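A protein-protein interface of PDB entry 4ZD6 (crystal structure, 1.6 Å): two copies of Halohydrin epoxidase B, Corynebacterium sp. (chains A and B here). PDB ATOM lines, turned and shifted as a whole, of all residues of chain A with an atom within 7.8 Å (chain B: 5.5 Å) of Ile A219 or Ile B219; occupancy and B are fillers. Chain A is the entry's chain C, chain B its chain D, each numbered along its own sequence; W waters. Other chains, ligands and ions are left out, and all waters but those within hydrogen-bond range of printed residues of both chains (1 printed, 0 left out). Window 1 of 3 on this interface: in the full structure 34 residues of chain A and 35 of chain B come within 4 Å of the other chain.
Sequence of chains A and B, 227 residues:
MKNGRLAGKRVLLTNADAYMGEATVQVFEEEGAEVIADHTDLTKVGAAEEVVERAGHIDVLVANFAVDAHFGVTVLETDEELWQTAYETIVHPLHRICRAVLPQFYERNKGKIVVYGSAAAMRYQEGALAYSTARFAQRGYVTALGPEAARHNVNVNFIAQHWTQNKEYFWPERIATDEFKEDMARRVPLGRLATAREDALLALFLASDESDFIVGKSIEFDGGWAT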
ATOM      1  N   VAL A 115      -2.075  -8.569  31.114  1.00  0.00           N
ATOM      2  CA  VAL A 115      -1.941  -7.149  30.804  1.00  0.00           C
ATOM      3  C   VAL A 115      -3.041  -6.778  29.823  1.00  0.00           C
ATOM      4  O   VAL A 115      -3.119  -7.345  28.730  1.00  0.00           O
ATOM      5  CB  VAL A 115      -0.563  -6.824  30.209  1.00  0.00           C
ATOM      6  CG1 VAL A 115      -0.448  -5.325  29.894  1.00  0.00           C
ATOM      7  CG2 VAL A 115       0.544  -7.295  31.146  1.00  0.00           C
ATOM      8  N   GLY A 117      -3.774  -4.570  27.180  1.00  0.00           N
ATOM      9  CA  GLY A 117      -2.981  -3.705  26.325  1.00  0.00           C
ATOM     10  C   GLY A 117      -3.800  -3.057  25.233  1.00  0.00           C
ATOM     11  O   GLY A 117      -4.870  -2.499  25.496  1.00  0.00           O
ATOM     12  N   SER A 118      -3.314  -3.132  24.000  1.00  0.00           N
ATOM     13  CA  SER A 118      -3.984  -2.475  22.889  1.00  0.00           C
ATOM     14  C   SER A 118      -3.557  -3.125  21.579  1.00  0.00           C
ATOM     15  O   SER A 118      -2.407  -3.543  21.418  1.00  0.00           O
ATOM     16  CB  SER A 118      -3.662  -0.977  22.865  1.00  0.00           C
ATOM     17  OG  SER A 118      -4.149  -0.368  21.680  1.00  0.00           O
ATOM     18  N   ALA A 119      -4.499  -3.184  20.637  1.00  0.00           N
ATOM     19  CA  ALA A 119      -4.173  -3.607  19.283  1.00  0.00           C
ATOM     20  C   ALA A 119      -3.289  -2.591  18.568  1.00  0.00           C
ATOM     21  O   ALA A 119      -2.686  -2.924  17.541  1.00  0.00           O
ATOM     22  CB  ALA A 119      -5.457  -3.837  18.477  1.00  0.00           C
ATOM     23  N   MET A 122       0.045  -3.756  17.876  1.00  0.00           N
ATOM     24  CA  MET A 122       0.174  -4.773  16.838  1.00  0.00           C
ATOM     25  C   MET A 122       0.232  -4.190  15.441  1.00  0.00           C
ATOM     26  O   MET A 122       1.008  -4.663  14.607  1.00  0.00           O
ATOM     27  CB  MET A 122      -1.001  -5.761  16.902  1.00  0.00           C
ATOM     28  CG  MET A 122      -1.280  -6.314  18.294  1.00  0.00           C
ATOM     29  SD  MET A 122       0.099  -7.248  19.012  1.00  0.00           S
ATOM     30  CE  MET A 122       0.448  -8.467  17.759  1.00  0.00           C
ATOM     31  N   ASN A 157       0.882 -12.623  29.875  1.00  0.00           N
ATOM     32  CA  ASN A 157       0.271 -12.490  28.561  1.00  0.00           C
ATOM     33  C   ASN A 157      -0.392 -11.126  28.402  1.00  0.00           C
ATOM     34  O   ASN A 157      -0.701 -10.441  29.379  1.00  0.00           O
ATOM     35  CB  ASN A 157      -0.739 -13.619  28.304  1.00  0.00           C
ATOM     36  CG  ASN A 157      -0.066 -14.974  28.198  1.00  0.00           C
ATOM     37  OD1 ASN A 157       0.668 -15.240  27.240  1.00  0.00           O
ATOM     38  ND2 ASN A 157      -0.281 -15.822  29.188  1.00  0.00           N
ATOM     39  N   PHE A 158      -0.601 -10.752  27.135  1.00  0.00           N
ATOM     40  CA  PHE A 158      -0.959  -9.401  26.708  1.00  0.00           C
ATOM     41  C   PHE A 158      -2.242  -9.482  25.892  1.00  0.00           C
ATOM     42  O   PHE A 158      -2.299 -10.213  24.899  1.00  0.00           O
ATOM     43  CB  PHE A 158       0.198  -8.813  25.879  1.00  0.00           C
ATOM     44  CG  PHE A 158      -0.007  -7.392  25.379  1.00  0.00           C
ATOM     45  CD1 PHE A 158       0.366  -6.299  26.150  1.00  0.00           C
ATOM     46  CD2 PHE A 158      -0.474  -7.156  24.090  1.00  0.00           C
ATOM     47  CE1 PHE A 158       0.222  -5.001  25.652  1.00  0.00           C
ATOM     48  CE2 PHE A 158      -0.613  -5.870  23.601  1.00  0.00           C
ATOM     49  CZ  PHE A 158      -0.267  -4.795  24.386  1.00  0.00           C
ATOM     50  N   ILE A 159      -3.277  -8.771  26.323  1.00  0.00           N
ATOM     51  CA  ILE A 159      -4.515  -8.681  25.550  1.00  0.00           C
ATOM     52  C   ILE A 159      -4.408  -7.439  24.676  1.00  0.00           C
ATOM     53  O   ILE A 159      -4.416  -6.316  25.180  1.00  0.00           O
ATOM     54  CB  ILE A 159      -5.754  -8.618  26.448  1.00  0.00           C
ATOM     55  CG1 ILE A 159      -5.893  -9.906  27.253  1.00  0.00           C
ATOM     56  CG2 ILE A 159      -7.007  -8.414  25.588  1.00  0.00           C
ATOM     57  CD1 ILE A 159      -7.041  -9.875  28.277  1.00  0.00           C
ATOM     58  N   ALA A 160      -4.338  -7.643  23.360  1.00  0.00           N
ATOM     59  CA  ALA A 160      -4.210  -6.539  22.406  1.00  0.00           C
ATOM     60  C   ALA A 160      -5.609  -6.125  21.953  1.00  0.00           C
ATOM     61  O   ALA A 160      -6.086  -6.486  20.874  1.00  0.00           O
ATOM     62  CB  ALA A 160      -3.332  -6.943  21.228  1.00  0.00           C
ATOM     63  N   GLN A 161      -6.271  -5.341  22.803  1.00  0.00           N
ATOM     64  CA  GLN A 161      -7.675  -5.023  22.590  1.00  0.00           C
ATOM     65  C   GLN A 161      -7.860  -3.743  21.780  1.00  0.00           C
ATOM     66  O   GLN A 161      -7.018  -2.840  21.763  1.00  0.00           O
ATOM     67  CB  GLN A 161      -8.408  -4.894  23.927  1.00  0.00           C
ATOM     68  CG  GLN A 161      -7.983  -3.683  24.737  1.00  0.00           C
ATOM     69  CD  GLN A 161      -8.717  -3.598  26.052  1.00  0.00           C
ATOM     70  OE1 GLN A 161      -8.394  -4.316  26.996  1.00  0.00           O
ATOM     71  NE2 GLN A 161      -9.712  -2.722  26.124  1.00  0.00           N
ATOM     72  N   HIS A 162      -9.016  -3.666  21.135  1.00  0.00           N
ATOM     73  CA  HIS A 162      -9.451  -2.496  20.395  1.00  0.00           C
ATOM     74  C   HIS A 162     -10.965  -2.597  20.294  1.00  0.00           C
ATOM     75  O   HIS A 162     -11.539  -3.678  20.458  1.00  0.00           O
ATOM     76  CB  HIS A 162      -8.792  -2.450  19.007  1.00  0.00           C
ATOM     77  CG  HIS A 162      -8.742  -1.087  18.388  1.00  0.00           C
ATOM     78  ND1 HIS A 162      -9.194   0.044  19.028  1.00  0.00           N
ATOM     79  CD2 HIS A 162      -8.280  -0.677  17.183  1.00  0.00           C
ATOM     80  CE1 HIS A 162      -9.026   1.093  18.240  1.00  0.00           C
ATOM     81  NE2 HIS A 162      -8.475   0.681  17.113  1.00  0.00           N
ATOM     82  N   ASP A 199     -14.184  -8.707  27.181  1.00  0.00           N
ATOM     83  CA  ASP A 199     -12.750  -8.534  27.402  1.00  0.00           C
ATOM     84  C   ASP A 199     -12.326  -9.227  28.693  1.00  0.00           C
ATOM     85  O   ASP A 199     -11.321  -9.952  28.731  1.00  0.00           O
ATOM     86  CB  ASP A 199     -12.457  -7.028  27.424  1.00  0.00           C
ATOM     87  CG  ASP A 199     -10.986  -6.681  27.313  1.00  0.00           C
ATOM     88  OD1 ASP A 199     -10.136  -7.546  27.014  1.00  0.00           O
ATOM     89  OD2 ASP A 199     -10.699  -5.485  27.499  1.00  0.00           O
ATOM     90  N   LEU A 202     -11.868 -12.961  28.355  1.00  0.00           N
ATOM     91  CA  LEU A 202     -10.557 -13.353  27.857  1.00  0.00           C
ATOM     92  C   LEU A 202      -9.528 -13.291  28.973  1.00  0.00           C
ATOM     93  O   LEU A 202      -8.725 -14.221  29.140  1.00  0.00           O
ATOM     94  CB  LEU A 202     -10.153 -12.463  26.678  1.00  0.00           C
ATOM     95  CG  LEU A 202      -8.722 -12.653  26.157  1.00  0.00           C
ATOM     96  CD1 LEU A 202      -8.462 -14.091  25.765  1.00  0.00           C
ATOM     97  CD2 LEU A 202      -8.455 -11.745  24.971  1.00  0.00           C
ATOM     98  N   PHE A 205      -9.865 -16.357  31.159  1.00  0.00           N
ATOM     99  CA  PHE A 205      -9.183 -17.526  30.618  1.00  0.00           C
ATOM    100  C   PHE A 205      -7.680 -17.455  30.888  1.00  0.00           C
ATOM    101  O   PHE A 205      -7.082 -18.421  31.379  1.00  0.00           O
ATOM    102  CB  PHE A 205      -9.470 -17.644  29.117  1.00  0.00           C
ATOM    103  CG  PHE A 205      -8.612 -18.649  28.422  1.00  0.00           C
ATOM    104  CD1 PHE A 205      -8.792 -20.004  28.648  1.00  0.00           C
ATOM    105  CD2 PHE A 205      -7.595 -18.243  27.567  1.00  0.00           C
ATOM    106  CE1 PHE A 205      -8.001 -20.948  28.015  1.00  0.00           C
ATOM    107  CE2 PHE A 205      -6.783 -19.185  26.946  1.00  0.00           C
ATOM    108  CZ  PHE A 205      -6.984 -20.536  27.166  1.00  0.00           C
ATOM    109  N   LEU A 206      -7.067 -16.297  30.606  1.00  0.00           N
ATOM    110  CA  LEU A 206      -5.622 -16.132  30.772  1.00  0.00           C
ATOM    111  C   LEU A 206      -5.191 -16.126  32.233  1.00  0.00           C
ATOM    112  O   LEU A 206      -4.014 -16.394  32.525  1.00  0.00           O
ATOM    113  CB  LEU A 206      -5.168 -14.835  30.092  1.00  0.00           C
ATOM    114  CG  LEU A 206      -5.330 -14.863  28.571  1.00  0.00           C
ATOM    115  CD1 LEU A 206      -5.057 -13.477  27.981  1.00  0.00           C
ATOM    116  CD2 LEU A 206      -4.407 -15.925  27.951  1.00  0.00           C
ATOM    117  N   SER A 211      -4.972 -22.077  31.205  1.00  0.00           N
ATOM    118  CA  SER A 211      -4.163 -21.399  30.194  1.00  0.00           C
ATOM    119  C   SER A 211      -2.671 -21.450  30.519  1.00  0.00           C
ATOM    120  O   SER A 211      -1.907 -20.593  30.050  1.00  0.00           O
ATOM    121  CB  SER A 211      -4.612 -19.945  30.036  1.00  0.00           C
ATOM    122  OG  SER A 211      -4.428 -19.224  31.249  1.00  0.00           O
ATOM    123  N   ILE A 214       0.190 -20.984  27.831  1.00  0.00           N
ATOM    124  CA  ILE A 214       0.246 -19.770  27.014  1.00  0.00           C
ATOM    125  C   ILE A 214       1.239 -18.816  27.664  1.00  0.00           C
ATOM    126  O   ILE A 214       1.070 -18.420  28.825  1.00  0.00           O
ATOM    127  CB  ILE A 214      -1.147 -19.148  26.847  1.00  0.00           C
ATOM    128  CG1 ILE A 214      -2.097 -20.175  26.204  1.00  0.00           C
ATOM    129  CG2 ILE A 214      -1.073 -17.887  25.996  1.00  0.00           C
ATOM    130  CD1 ILE A 214      -3.524 -19.710  26.102  1.00  0.00           C
ATOM    131  N   GLY A 216       3.834 -15.465  27.189  1.00  0.00           N
ATOM    132  CA  GLY A 216       4.384 -14.287  26.527  1.00  0.00           C
ATOM    133  C   GLY A 216       3.678 -13.901  25.244  1.00  0.00           C
ATOM    134  O   GLY A 216       4.296 -13.303  24.353  1.00  0.00           O
ATOM    135  N   LYS A 217       2.394 -14.215  25.133  1.00  0.00           N
ATOM    136  CA  LYS A 217       1.646 -14.052  23.900  1.00  0.00           C
ATOM    137  C   LYS A 217       0.837 -12.759  23.898  1.00  0.00           C
ATOM    138  O   LYS A 217       0.452 -12.233  24.948  1.00  0.00           O
ATOM    139  CB  LYS A 217       0.708 -15.240  23.679  1.00  0.00           C
ATOM    140  CG  LYS A 217       1.414 -16.592  23.629  1.00  0.00           C
ATOM    141  CD  LYS A 217       2.550 -16.600  22.605  1.00  0.00           C
ATOM    142  CE  LYS A 217       3.261 -17.951  22.657  1.00  0.00           C
ATOM    143  NZ  LYS A 217       4.375 -18.095  21.687  1.00  0.00           N
ATOM    144  N   SER A 218       0.605 -12.243  22.698  1.00  0.00           N
ATOM    145  CA  SER A 218      -0.341 -11.164  22.467  1.00  0.00           C
ATOM    146  C   SER A 218      -1.555 -11.745  21.762  1.00  0.00           C
ATOM    147  O   SER A 218      -1.444 -12.223  20.628  1.00  0.00           O
ATOM    148  CB  SER A 218       0.282 -10.052  21.621  1.00  0.00           C
ATOM    149  OG  SER A 218       1.507  -9.617  22.167  1.00  0.00           O
ATOM    150  N   ILE A 219      -2.707 -11.697  22.420  1.00  0.00           N
ATOM    151  CA  ILE A 219      -3.953 -12.188  21.850  1.00  0.00           C
ATOM    152  C   ILE A 219      -4.766 -10.989  21.392  1.00  0.00           C
ATOM    153  O   ILE A 219      -5.119 -10.122  22.203  1.00  0.00           O
ATOM    154  CB  ILE A 219      -4.735 -13.033  22.862  1.00  0.00           C
ATOM    155  CG1 ILE A 219      -3.886 -14.213  23.325  1.00  0.00           C
ATOM    156  CG2 ILE A 219      -6.010 -13.540  22.223  1.00  0.00           C
ATOM    157  CD1 ILE A 219      -4.530 -14.980  24.436  1.00  0.00           C
ATOM    158  N   GLU A 220      -5.051 -10.923  20.090  1.00  0.00           N
ATOM    159  CA  GLU A 220      -5.718  -9.751  19.530  1.00  0.00           C
ATOM    160  C   GLU A 220      -7.213  -9.844  19.777  1.00  0.00           C
ATOM    161  O   GLU A 220      -7.865 -10.789  19.328  1.00  0.00           O
ATOM    162  CB  GLU A 220      -5.438  -9.613  18.039  1.00  0.00           C
ATOM    163  CG  GLU A 220      -4.041  -9.104  17.771  1.00  0.00           C
ATOM    164  CD  GLU A 220      -3.549  -9.415  16.379  1.00  0.00           C
ATOM    165  OE1 GLU A 220      -4.374  -9.552  15.449  1.00  0.00           O
ATOM    166  OE2 GLU A 220      -2.318  -9.527  16.221  1.00  0.00           O
ATOM    167  N   PHE A 221      -7.740  -8.865  20.499  1.00  0.00           N
ATOM    168  CA  PHE A 221      -9.132  -8.820  20.923  1.00  0.00           C
ATOM    169  C   PHE A 221      -9.736  -7.595  20.253  1.00  0.00           C
ATOM    170  O   PHE A 221      -9.799  -6.517  20.833  1.00  0.00           O
ATOM    171  CB  PHE A 221      -9.210  -8.757  22.470  1.00  0.00           C
ATOM    172  CG  PHE A 221     -10.603  -8.734  23.001  1.00  0.00           C
ATOM    173  CD1 PHE A 221     -11.305  -9.916  23.183  1.00  0.00           C
ATOM    174  CD2 PHE A 221     -11.219  -7.524  23.308  1.00  0.00           C
ATOM    175  CE1 PHE A 221     -12.610  -9.880  23.657  1.00  0.00           C
ATOM    176  CE2 PHE A 221     -12.510  -7.495  23.793  1.00  0.00           C
ATOM    177  CZ  PHE A 221     -13.200  -8.673  23.963  1.00  0.00           C
ATOM    178  N   ASP A 222     -10.161  -7.759  19.001  1.00  0.00           N
ATOM    179  CA  ASP A 222     -10.440  -6.570  18.203  1.00  0.00           C
ATOM    180  C   ASP A 222     -11.503  -6.789  17.133  1.00  0.00           C
ATOM    181  O   ASP A 222     -11.571  -5.993  16.191  1.00  0.00           O
ATOM    182  CB  ASP A 222      -9.132  -6.052  17.550  1.00  0.00           C
ATOM    183  CG  ASP A 222      -8.555  -7.006  16.508  1.00  0.00           C
ATOM    184  OD1 ASP A 222      -9.159  -8.052  16.202  1.00  0.00           O
ATOM    185  OD2 ASP A 222      -7.469  -6.684  15.968  1.00  0.00           O
ATOM    186  N   PHE B 158      -7.566 -20.173  14.815  1.00  0.00           N
ATOM    187  CA  PHE B 158      -6.503 -21.132  14.526  1.00  0.00           C
ATOM    188  C   PHE B 158      -5.646 -21.298  15.774  1.00  0.00           C
ATOM    189  O   PHE B 158      -5.104 -20.313  16.285  1.00  0.00           O
ATOM    190  CB  PHE B 158      -5.678 -20.606  13.340  1.00  0.00           C
ATOM    191  CG  PHE B 158      -4.530 -21.489  12.894  1.00  0.00           C
ATOM    192  CD1 PHE B 158      -4.725 -22.505  11.966  1.00  0.00           C
ATOM    193  CD2 PHE B 158      -3.233 -21.226  13.326  1.00  0.00           C
ATOM    194  CE1 PHE B 158      -3.663 -23.268  11.504  1.00  0.00           C
ATOM    195  CE2 PHE B 158      -2.164 -21.984  12.874  1.00  0.00           C
ATOM    196  CZ  PHE B 158      -2.368 -23.011  11.961  1.00  0.00           C
ATOM    197  N   ILE B 159      -5.527 -22.530  16.266  1.00  0.00           N
ATOM    198  CA  ILE B 159      -4.645 -22.831  17.394  1.00  0.00           C
ATOM    199  C   ILE B 159      -3.289 -23.239  16.832  1.00  0.00           C
ATOM    200  O   ILE B 159      -3.163 -24.285  16.189  1.00  0.00           O
ATOM    201  CB  ILE B 159      -5.226 -23.930  18.289  1.00  0.00           C
ATOM    202  CG1 ILE B 159      -6.546 -23.455  18.917  1.00  0.00           C
ATOM    203  CG2 ILE B 159      -4.202 -24.335  19.373  1.00  0.00           C
ATOM    204  CD1 ILE B 159      -7.243 -24.534  19.726  1.00  0.00           C
ATOM    205  N   ALA B 160      -2.261 -22.417  17.075  1.00  0.00           N
ATOM    206  CA  ALA B 160      -0.932 -22.705  16.527  1.00  0.00           C
ATOM    207  C   ALA B 160      -0.147 -23.469  17.585  1.00  0.00           C
ATOM    208  O   ALA B 160       0.676 -22.912  18.315  1.00  0.00           O
ATOM    209  CB  ALA B 160      -0.217 -21.420  16.123  1.00  0.00           C
ATOM    210  N   GLN B 161      -0.416 -24.773  17.666  1.00  0.00           N
ATOM    211  CA  GLN B 161       0.118 -25.576  18.757  1.00  0.00           C
ATOM    212  C   GLN B 161       1.482 -26.171  18.430  1.00  0.00           C
ATOM    213  O   GLN B 161       1.840 -26.393  17.273  1.00  0.00           O
ATOM    214  CB  GLN B 161      -0.841 -26.700  19.137  1.00  0.00           C
ATOM    215  CG  GLN B 161      -0.993 -27.754  18.069  1.00  0.00           C
ATOM    216  CD  GLN B 161      -2.016 -28.786  18.477  1.00  0.00           C
ATOM    217  OE1 GLN B 161      -3.210 -28.501  18.493  1.00  0.00           O
ATOM    218  NE2 GLN B 161      -1.553 -29.989  18.802  1.00  0.00           N
ATOM    219  N   LEU B 202      -8.210 -24.627  25.462  1.00  0.00           N
ATOM    220  CA  LEU B 202      -8.136 -23.462  24.588  1.00  0.00           C
ATOM    221  C   LEU B 202      -9.187 -23.542  23.492  1.00  0.00           C
ATOM    222  O   LEU B 202      -9.868 -22.551  23.201  1.00  0.00           O
ATOM    223  CB  LEU B 202      -6.735 -23.345  23.976  1.00  0.00           C
ATOM    224  CG  LEU B 202      -6.553 -22.268  22.903  1.00  0.00           C
ATOM    225  CD1 LEU B 202      -6.959 -20.922  23.436  1.00  0.00           C
ATOM    226  CD2 LEU B 202      -5.105 -22.241  22.431  1.00  0.00           C
ATOM    227  N   LEU B 206     -12.413 -20.967  22.576  1.00  0.00           N
ATOM    228  CA  LEU B 206     -12.668 -20.449  21.236  1.00  0.00           C
ATOM    229  C   LEU B 206     -13.957 -20.980  20.624  1.00  0.00           C
ATOM    230  O   LEU B 206     -14.488 -20.348  19.709  1.00  0.00           O
ATOM    231  CB  LEU B 206     -11.478 -20.756  20.329  1.00  0.00           C
ATOM    232  CG  LEU B 206     -10.146 -20.083  20.694  1.00  0.00           C
ATOM    233  CD1 LEU B 206      -9.021 -20.675  19.860  1.00  0.00           C
ATOM    234  CD2 LEU B 206     -10.230 -18.557  20.495  1.00  0.00           C
ATOM    235  N   ILE B 214     -13.206 -12.694  19.084  1.00  0.00           N
ATOM    236  CA  ILE B 214     -11.946 -13.192  18.526  1.00  0.00           C
ATOM    237  C   ILE B 214     -12.204 -13.655  17.095  1.00  0.00           C
ATOM    238  O   ILE B 214     -12.966 -14.601  16.873  1.00  0.00           O
ATOM    239  CB  ILE B 214     -11.372 -14.335  19.381  1.00  0.00           C
ATOM    240  CG1 ILE B 214     -11.413 -13.968  20.864  1.00  0.00           C
ATOM    241  CG2 ILE B 214      -9.939 -14.647  18.968  1.00  0.00           C
ATOM    242  CD1 ILE B 214     -10.502 -12.846  21.229  1.00  0.00           C
ATOM    243  N   LYS B 217      -7.939 -15.238  14.219  1.00  0.00           N
ATOM    244  CA  LYS B 217      -6.692 -15.112  14.957  1.00  0.00           C
ATOM    245  C   LYS B 217      -5.943 -16.438  15.020  1.00  0.00           C
ATOM    246  O   LYS B 217      -6.535 -17.518  14.986  1.00  0.00           O
ATOM    247  CB  LYS B 217      -6.941 -14.613  16.383  1.00  0.00           C
ATOM    248  CG  LYS B 217      -7.634 -13.266  16.468  1.00  0.00           C
ATOM    249  CD  LYS B 217      -6.978 -12.237  15.565  1.00  0.00           C
ATOM    250  CE  LYS B 217      -7.768 -10.930  15.611  1.00  0.00           C
ATOM    251  NZ  LYS B 217      -7.151  -9.786  14.889  1.00  0.00           N
ATOM    252  N   SER B 218      -4.616 -16.332  15.094  1.00  0.00           N
ATOM    253  CA  SER B 218      -3.735 -17.456  15.376  1.00  0.00           C
ATOM    254  C   SER B 218      -3.276 -17.311  16.820  1.00  0.00           C
ATOM    255  O   SER B 218      -2.614 -16.326  17.160  1.00  0.00           O
ATOM    256  CB  SER B 218      -2.529 -17.474  14.432  1.00  0.00           C
ATOM    257  OG  SER B 218      -2.912 -17.481  13.070  1.00  0.00           O
ATOM    258  N   ILE B 219      -3.659 -18.254  17.673  1.00  0.00           N
ATOM    259  CA  ILE B 219      -3.248 -18.244  19.075  1.00  0.00           C
ATOM    260  C   ILE B 219      -2.120 -19.251  19.253  1.00  0.00           C
ATOM    261  O   ILE B 219      -2.305 -20.455  19.025  1.00  0.00           O
ATOM    262  CB  ILE B 219      -4.411 -18.578  20.023  1.00  0.00           C
ATOM    263  CG1 ILE B 219      -5.688 -17.812  19.651  1.00  0.00           C
ATOM    264  CG2 ILE B 219      -3.997 -18.249  21.451  1.00  0.00           C
ATOM    265  CD1 ILE B 219      -5.703 -16.377  20.086  1.00  0.00           C
ATOM    266  N   GLU B 220      -0.959 -18.767  19.688  1.00  0.00           N
ATOM    267  CA  GLU B 220       0.214 -19.620  19.833  1.00  0.00           C
ATOM    268  C   GLU B 220       0.140 -20.417  21.127  1.00  0.00           C
ATOM    269  O   GLU B 220       0.115 -19.844  22.222  1.00  0.00           O
ATOM    270  CB  GLU B 220       1.479 -18.776  19.795  1.00  0.00           C
ATOM    271  CG  GLU B 220       1.846 -18.389  18.379  1.00  0.00           C
ATOM    272  CD  GLU B 220       2.751 -17.186  18.321  1.00  0.00           C
ATOM    273  OE1 GLU B 220       3.670 -17.085  19.164  1.00  0.00           O
ATOM    274  OE2 GLU B 220       2.524 -16.323  17.440  1.00  0.00           O
ATOM    275  N   PHE B 221       0.123 -21.738  20.993  1.00  0.00           N
ATOM    276  CA  PHE B 221      -0.062 -22.668  22.099  1.00  0.00           C
ATOM    277  C   PHE B 221       1.177 -23.548  22.105  1.00  0.00           C
ATOM    278  O   PHE B 221       1.186 -24.618  21.501  1.00  0.00           O
ATOM    279  CB  PHE B 221      -1.380 -23.484  21.909  1.00  0.00           C
ATOM    280  CG  PHE B 221      -1.684 -24.421  23.041  1.00  0.00           C
ATOM    281  CD1 PHE B 221      -2.271 -23.949  24.211  1.00  0.00           C
ATOM    282  CD2 PHE B 221      -1.377 -25.769  22.942  1.00  0.00           C
ATOM    283  CE1 PHE B 221      -2.545 -24.817  25.260  1.00  0.00           C
ATOM    284  CE2 PHE B 221      -1.650 -26.637  23.985  1.00  0.00           C
ATOM    285  CZ  PHE B 221      -2.234 -26.157  25.146  1.00  0.00           C
HETATM  286  O   HOH W   1      -2.708 -14.574  19.607  1.00  0.00           O
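O of Phe A158 lies within hydrogen-bond range of N of Ile A219, at 2.9 Å.
N of Ala A160 is in hydrogen-bond range of O of Ile A219, 2.8 Å away.
N of His A162 is in hydrogen-bond range of O of Phe A221 (3.0 Å).
OG of Ser A211 lies within hydrogen-bond range of O of Phe A205 (2.8 Å).
The backbone carbonyl oxygen (O) of Phe B158 lies within hydrogen-bond range of the backbone NH (N) of Ile B219 (2.9 Å).
The backbone carbonyl oxygen (O) of Ile B219 lies within hydrogen-bond range of the backbone NH (N) of Ala B160 (2.8 Å).
Ile A219 touches just one residue of chain B: Ile B219 (3.6 Å).
Of the printed residues of chain A, Leu B202 touches Phe A205.
Of chain A, only Ile A219 comes within 4 Å of Ile B219.
Printed residues of chain A within 4 Å of Glu B220: Lys A217 (2.8 Å).
The nearest residue of chain B that does not touch Ile A219 is Ile B214 (4.7 Å).
The nearest printed residue of chain B that does not touch Lys A217 is Phe B221 (5.2 Å).
Water W1 bridges the backbone carbonyl oxygen of Ser A218 (2.9 Å) and the backbone carbonyl oxygen of Ser B218 (3.0 Å).
Leu B202 touches Phe A205 (CD1 to CZ, 3.8 Å).
Ile B219 touches Ile A219.
O of Glu A220 touches CD1 of Ile B214, 3.8 Å away.
Phe A221 touches Ile B214.
Of the 12 printed residues of chain B, 5 touch a printed residue of chain A.
Hydrophobic or aromatic side chains of chain B within 4 Å of the printed part of chain A: Leu B202, Ile B214 and Ile B219.
Of the 24 printed residues of chain A, 6 touch a printed residue of chain B.
Among the printed residues, Asp or Glu carboxylates within 4 Å of a Lys or Arg side-chain nitrogen of the other chain: Lys A217 with Glu B220, Glu A220 with Lys B217 and Asp A222 with Lys B217.
Lys A217 touches Glu B220, and with the chains exchanged Glu A220 touches Lys B217.
Ile A219 touches its own counterpart, Ile B219.
Glu A220 touches Ile B214, but with the chains exchanged Ile A214 does not touch Glu B220 (4.4 Å).
Phe A221 touches Ile B214, but with the chains exchanged Ile A214 does not touch Phe B221 (4.3 Å).
Of the 7 pairs that touch across the chains among the printed residues, 3 have their exchanged pair printed and touching as well.
OE1 of Glu B220 lies within salt-bridge range of NZ of Lys A217 (2.8 Å).
OE1 of Glu A220 lies within salt-bridge range of NZ of Lys B217 (2.8 Å).
The side-chain carboxylate (OD1) of Asp A222 is in salt-bridge range of the side-chain amino group (NZ) of Lys B217.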
